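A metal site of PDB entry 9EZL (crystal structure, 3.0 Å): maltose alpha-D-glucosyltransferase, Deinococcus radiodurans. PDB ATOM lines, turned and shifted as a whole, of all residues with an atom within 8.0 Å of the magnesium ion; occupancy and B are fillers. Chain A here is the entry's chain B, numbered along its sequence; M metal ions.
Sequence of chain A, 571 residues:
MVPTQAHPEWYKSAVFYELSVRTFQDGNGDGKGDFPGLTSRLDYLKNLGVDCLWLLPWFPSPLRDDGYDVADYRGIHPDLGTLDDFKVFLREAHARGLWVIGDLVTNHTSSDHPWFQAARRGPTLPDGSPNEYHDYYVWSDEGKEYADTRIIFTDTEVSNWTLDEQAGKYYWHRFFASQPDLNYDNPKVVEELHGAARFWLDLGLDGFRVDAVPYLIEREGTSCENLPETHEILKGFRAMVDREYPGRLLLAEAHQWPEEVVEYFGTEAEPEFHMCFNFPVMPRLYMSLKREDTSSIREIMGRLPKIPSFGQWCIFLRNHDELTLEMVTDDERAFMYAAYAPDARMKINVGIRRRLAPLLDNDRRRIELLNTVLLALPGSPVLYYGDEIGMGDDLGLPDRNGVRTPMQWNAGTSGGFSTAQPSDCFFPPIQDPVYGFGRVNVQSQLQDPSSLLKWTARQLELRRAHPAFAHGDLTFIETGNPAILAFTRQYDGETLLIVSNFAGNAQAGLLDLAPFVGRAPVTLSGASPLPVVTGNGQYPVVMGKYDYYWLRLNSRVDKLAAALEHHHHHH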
ATOM      1  N   VAL A  21     -34.613  18.909  26.057  1.00  0.00           N
ATOM      2  CA  VAL A  21     -33.359  18.681  25.340  1.00  0.00           C
ATOM      3  C   VAL A  21     -32.805  20.002  24.821  1.00  0.00           C
ATOM      4  O   VAL A  21     -31.598  20.255  24.891  1.00  0.00           O
ATOM      5  CB  VAL A  21     -33.553  17.668  24.194  1.00  0.00           C
ATOM      6  CG1 VAL A  21     -32.531  17.877  23.078  1.00  0.00           C
ATOM      7  CG2 VAL A  21     -33.466  16.264  24.717  1.00  0.00           C
ATOM      8  N   ARG A  22     -33.685  20.856  24.304  1.00  0.00           N
ATOM      9  CA  ARG A  22     -33.240  22.101  23.683  1.00  0.00           C
ATOM     10  C   ARG A  22     -32.494  23.002  24.665  1.00  0.00           C
ATOM     11  O   ARG A  22     -31.716  23.858  24.219  1.00  0.00           O
ATOM     12  CB  ARG A  22     -34.425  22.847  23.056  1.00  0.00           C
ATOM     13  CG  ARG A  22     -33.988  23.864  22.036  1.00  0.00           C
ATOM     14  CD  ARG A  22     -35.142  24.465  21.320  1.00  0.00           C
ATOM     15  NE  ARG A  22     -35.479  23.695  20.121  1.00  0.00           N
ATOM     16  CZ  ARG A  22     -36.461  22.810  20.051  1.00  0.00           C
ATOM     17  NH1 ARG A  22     -37.270  22.582  21.085  1.00  0.00           N
ATOM     18  NH2 ARG A  22     -36.644  22.135  18.918  1.00  0.00           N
ATOM     19  N   GLN A  25     -28.109  20.303  27.271  1.00  0.00           N
ATOM     20  CA  GLN A  25     -26.707  20.318  26.911  1.00  0.00           C
ATOM     21  C   GLN A  25     -26.604  20.433  25.392  1.00  0.00           C
ATOM     22  O   GLN A  25     -27.303  19.720  24.673  1.00  0.00           O
ATOM     23  CB  GLN A  25     -25.977  19.058  27.398  1.00  0.00           C
ATOM     24  CG  GLN A  25     -24.473  19.057  27.108  1.00  0.00           C
ATOM     25  CD  GLN A  25     -23.708  20.100  27.913  1.00  0.00           C
ATOM     26  OE1 GLN A  25     -23.539  19.968  29.125  1.00  0.00           O
ATOM     27  NE2 GLN A  25     -23.262  21.156  27.230  1.00  0.00           N
ATOM     28  N   ASP A  26     -25.757  21.341  24.932  1.00  0.00           N
ATOM     29  CA  ASP A  26     -25.431  21.477  23.532  1.00  0.00           C
ATOM     30  C   ASP A  26     -24.167  20.664  23.228  1.00  0.00           C
ATOM     31  O   ASP A  26     -23.233  20.630  24.019  1.00  0.00           O
ATOM     32  CB  ASP A  26     -25.235  22.952  23.187  1.00  0.00           C
ATOM     33  CG  ASP A  26     -25.043  23.183  21.691  1.00  0.00           C
ATOM     34  OD1 ASP A  26     -25.427  22.303  20.866  1.00  0.00           O
ATOM     35  OD2 ASP A  26     -24.521  24.273  21.354  1.00  0.00           O
ATOM     36  N   GLY A  27     -24.156  19.993  22.082  1.00  0.00           N
ATOM     37  CA  GLY A  27     -22.984  19.226  21.727  1.00  0.00           C
ATOM     38  C   GLY A  27     -22.058  19.911  20.742  1.00  0.00           C
ATOM     39  O   GLY A  27     -20.842  19.684  20.739  1.00  0.00           O
ATOM     40  N   ASN A  28     -22.625  20.782  19.908  1.00  0.00           N
ATOM     41  CA  ASN A  28     -21.885  21.267  18.747  1.00  0.00           C
ATOM     42  C   ASN A  28     -21.738  22.790  18.703  1.00  0.00           C
ATOM     43  O   ASN A  28     -21.229  23.319  17.701  1.00  0.00           O
ATOM     44  CB  ASN A  28     -22.570  20.771  17.468  1.00  0.00           C
ATOM     45  CG  ASN A  28     -24.049  21.074  17.456  1.00  0.00           C
ATOM     46  OD1 ASN A  28     -24.686  21.080  18.505  1.00  0.00           O
ATOM     47  ND2 ASN A  28     -24.600  21.324  16.282  1.00  0.00           N
ATOM     48  N   GLY A  29     -22.146  23.515  19.747  1.00  0.00           N
ATOM     49  CA  GLY A  29     -21.930  24.957  19.800  1.00  0.00           C
ATOM     50  C   GLY A  29     -22.814  25.801  18.910  1.00  0.00           C
ATOM     51  O   GLY A  29     -22.511  26.980  18.739  1.00  0.00           O
ATOM     52  N   ASP A  30     -23.881  25.223  18.336  1.00  0.00           N
ATOM     53  CA  ASP A  30     -24.903  25.934  17.563  1.00  0.00           C
ATOM     54  C   ASP A  30     -25.907  26.678  18.441  1.00  0.00           C
ATOM     55  O   ASP A  30     -26.846  27.277  17.904  1.00  0.00           O
ATOM     56  CB  ASP A  30     -25.680  24.982  16.642  1.00  0.00           C
ATOM     57  CG  ASP A  30     -26.502  23.923  17.403  1.00  0.00           C
ATOM     58  OD1 ASP A  30     -26.229  23.653  18.602  1.00  0.00           O
ATOM     59  OD2 ASP A  30     -27.427  23.336  16.798  1.00  0.00           O
ATOM     60  N   GLY A  31     -25.736  26.642  19.769  1.00  0.00           N
ATOM     61  CA  GLY A  31     -26.578  27.371  20.695  1.00  0.00           C
ATOM     62  C   GLY A  31     -27.795  26.621  21.221  1.00  0.00           C
ATOM     63  O   GLY A  31     -28.462  27.126  22.139  1.00  0.00           O
ATOM     64  N   LYS A  32     -28.113  25.447  20.673  1.00  0.00           N
ATOM     65  CA  LYS A  32     -29.324  24.741  21.083  1.00  0.00           C
ATOM     66  C   LYS A  32     -29.000  23.319  21.478  1.00  0.00           C
ATOM     67  O   LYS A  32     -28.362  22.591  20.707  1.00  0.00           O
ATOM     68  CB  LYS A  32     -30.387  24.749  19.987  1.00  0.00           C
ATOM     69  CG  LYS A  32     -30.082  25.656  18.842  1.00  0.00           C
ATOM     70  CD  LYS A  32     -31.313  25.837  18.000  1.00  0.00           C
ATOM     71  CE  LYS A  32     -31.023  26.745  16.829  1.00  0.00           C
ATOM     72  NZ  LYS A  32     -29.972  26.149  15.963  1.00  0.00           N
ATOM     73  N   GLY A  33     -29.460  22.929  22.672  1.00  0.00           N
ATOM     74  CA  GLY A  33     -29.189  21.598  23.189  1.00  0.00           C
ATOM     75  C   GLY A  33     -29.719  20.513  22.279  1.00  0.00           C
ATOM     76  O   GLY A  33     -30.693  20.704  21.548  1.00  0.00           O
ATOM     77  N   ASP A  34     -29.078  19.343  22.349  1.00  0.00           N
ATOM     78  CA  ASP A  34     -29.338  18.255  21.408  1.00  0.00           C
ATOM     79  C   ASP A  34     -29.173  16.906  22.094  1.00  0.00           C
ATOM     80  O   ASP A  34     -28.791  16.829  23.273  1.00  0.00           O
ATOM     81  CB  ASP A  34     -28.440  18.375  20.175  1.00  0.00           C
ATOM     82  CG  ASP A  34     -27.056  18.960  20.498  1.00  0.00           C
ATOM     83  OD1 ASP A  34     -26.253  18.284  21.197  1.00  0.00           O
ATOM     84  OD2 ASP A  34     -26.764  20.090  20.048  1.00  0.00           O
ATOM     85  N   PHE A  35     -29.474  15.834  21.357  1.00  0.00           N
ATOM     86  CA  PHE A  35     -29.441  14.474  21.899  1.00  0.00           C
ATOM     87  C   PHE A  35     -28.023  13.982  22.111  1.00  0.00           C
ATOM     88  O   PHE A  35     -27.782  13.277  23.101  1.00  0.00           O
ATOM     89  CB  PHE A  35     -30.194  13.502  21.010  1.00  0.00           C
ATOM     90  CG  PHE A  35     -31.661  13.583  21.202  1.00  0.00           C
ATOM     91  CD1 PHE A  35     -32.271  12.884  22.232  1.00  0.00           C
ATOM     92  CD2 PHE A  35     -32.418  14.424  20.414  1.00  0.00           C
ATOM     93  CE1 PHE A  35     -33.623  12.985  22.430  1.00  0.00           C
ATOM     94  CE2 PHE A  35     -33.777  14.535  20.605  1.00  0.00           C
ATOM     95  CZ  PHE A  35     -34.383  13.821  21.609  1.00  0.00           C
ATOM     96  N   PRO A  36     -27.079  14.289  21.210  1.00  0.00           N
ATOM     97  CA  PRO A  36     -25.654  14.121  21.573  1.00  0.00           C
ATOM     98  C   PRO A  36     -25.283  14.762  22.900  1.00  0.00           C
ATOM     99  O   PRO A  36     -24.721  14.101  23.786  1.00  0.00           O
ATOM    100  CB  PRO A  36     -24.948  14.777  20.400  1.00  0.00           C
ATOM    101  CG  PRO A  36     -25.834  14.502  19.281  1.00  0.00           C
ATOM    102  CD  PRO A  36     -27.212  14.687  19.802  1.00  0.00           C
ATOM    103  N   GLY A  37     -25.582  16.053  23.045  1.00  0.00           N
ATOM    104  CA  GLY A  37     -25.360  16.726  24.316  1.00  0.00           C
ATOM    105  C   GLY A  37     -25.948  15.967  25.481  1.00  0.00           C
ATOM    106  O   GLY A  37     -25.253  15.696  26.463  1.00  0.00           O
ATOM    107  N   PRO A  78     -34.983  19.047  13.948  1.00  0.00           N
ATOM    108  CA  PRO A  78     -33.592  19.296  13.555  1.00  0.00           C
ATOM    109  C   PRO A  78     -32.748  19.852  14.681  1.00  0.00           C
ATOM    110  O   PRO A  78     -31.731  19.249  15.004  1.00  0.00           O
ATOM    111  CB  PRO A  78     -33.722  20.313  12.410  1.00  0.00           C
ATOM    112  CG  PRO A  78     -35.225  20.446  12.122  1.00  0.00           C
ATOM    113  CD  PRO A  78     -35.914  19.345  12.855  1.00  0.00           C
ATOM    114  N   ASP A  79     -33.207  20.948  15.329  1.00  0.00           N
ATOM    115  CA  ASP A  79     -32.547  21.598  16.466  1.00  0.00           C
ATOM    116  C   ASP A  79     -31.944  20.631  17.482  1.00  0.00           C
ATOM    117  O   ASP A  79     -30.948  20.966  18.133  1.00  0.00           O
ATOM    118  CB  ASP A  79     -33.505  22.537  17.209  1.00  0.00           C
ATOM    119  CG  ASP A  79     -33.657  23.888  16.527  1.00  0.00           C
ATOM    120  OD1 ASP A  79     -33.044  24.097  15.472  1.00  0.00           O
ATOM    121  OD2 ASP A  79     -34.359  24.772  17.085  1.00  0.00           O
ATOM    122  N   LEU A  80     -32.523  19.425  17.607  1.00  0.00           N
ATOM    123  CA  LEU A  80     -32.149  18.464  18.645  1.00  0.00           C
ATOM    124  C   LEU A  80     -31.283  17.310  18.139  1.00  0.00           C
ATOM    125  O   LEU A  80     -30.725  16.566  18.957  1.00  0.00           O
ATOM    126  CB  LEU A  80     -33.420  17.890  19.284  1.00  0.00           C
ATOM    127  CG  LEU A  80     -34.466  18.937  19.623  1.00  0.00           C
ATOM    128  CD1 LEU A  80     -35.601  18.281  20.346  1.00  0.00           C
ATOM    129  CD2 LEU A  80     -33.865  20.052  20.484  1.00  0.00           C
ATOM    130  N   GLY A  81     -31.132  17.127  16.837  1.00  0.00           N
ATOM    131  CA  GLY A  81     -30.345  16.071  16.251  1.00  0.00           C
ATOM    132  C   GLY A  81     -31.193  15.255  15.338  1.00  0.00           C
ATOM    133  O   GLY A  81     -32.306  15.651  14.959  1.00  0.00           O
ATOM    134  N   PHE A 417     -23.375  25.221  29.044  1.00  0.00           N
ATOM    135  CA  PHE A 417     -24.436  24.681  28.195  1.00  0.00           C
ATOM    136  C   PHE A 417     -23.971  24.601  26.748  1.00  0.00           C
ATOM    137  O   PHE A 417     -24.140  23.574  26.089  1.00  0.00           O
ATOM    138  CB  PHE A 417     -25.698  25.536  28.328  1.00  0.00           C
ATOM    139  CG  PHE A 417     -26.696  25.361  27.181  1.00  0.00           C
ATOM    140  CD1 PHE A 417     -27.477  24.221  27.087  1.00  0.00           C
ATOM    141  CD2 PHE A 417     -26.856  26.369  26.222  1.00  0.00           C
ATOM    142  CE1 PHE A 417     -28.406  24.069  26.040  1.00  0.00           C
ATOM    143  CE2 PHE A 417     -27.767  26.220  25.187  1.00  0.00           C
ATOM    144  CZ  PHE A 417     -28.545  25.070  25.092  1.00  0.00           C
ATOM    145  N   SER A 418     -23.349  25.665  26.244  1.00  0.00           N
ATOM    146  CA  SER A 418     -22.855  25.685  24.875  1.00  0.00           C
ATOM    147  C   SER A 418     -21.540  26.441  24.830  1.00  0.00           C
ATOM    148  O   SER A 418     -21.207  27.206  25.748  1.00  0.00           O
ATOM    149  CB  SER A 418     -23.866  26.336  23.924  1.00  0.00           C
ATOM    150  OG  SER A 418     -23.322  26.506  22.622  1.00  0.00           O
HETATM  151 MG    MG M   1     -26.865  21.798  19.153  1.00  0.00          MG
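OD1 of Asp 34 sits at hydrogen-bond distance from N of Gly 27, 2.8 Å away.
The backbone carbonyl oxygen of Gln 25 is in hydrogen-bond range of the backbone NH of Asp 34, 2.9 Å away.
The side-chain carboxylate of Asp 34 is in hydrogen-bond range of the backbone NH of Gly 37 (3.0 Å).
N of Gly 31 lies within hydrogen-bond range of OD2 of Asp 26 (3.1 Å).
The backbone NH of Gly 29 sits at hydrogen-bond distance from the side-chain carboxylate of Asp 26 (3.0 Å).
OG of Ser 418 lies within hydrogen-bond range of OD2 of Asp 26.
The backbone NH (N) of Asp 26 is in hydrogen-bond range of the backbone carbonyl oxygen (O) of Phe 417 (3.0 Å).
NZ of Lys 32 is in salt-bridge range of OD1 of Asp 79.
Five residues have an atom within 4 Å of the magnesium ion: Asp 26, Asn 28, Asp 30, Lys 32 and Asp 34.
The magnesium ion is bound by the side-chain carboxylate (OD2) of Asp 34 (1.9 Å), the side-chain carboxylate (OD1) of Asp 30 (2.0 Å), the side-chain carboxylate (OD1) of Asp 26 (2.3 Å), the backbone carbonyl oxygen (O) of Lys 32 (2.3 Å) and the side-chain amide oxygen (OD1) of Asn 28 (2.4 Å).
The magnesium ion has five donor atoms within binding distance.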
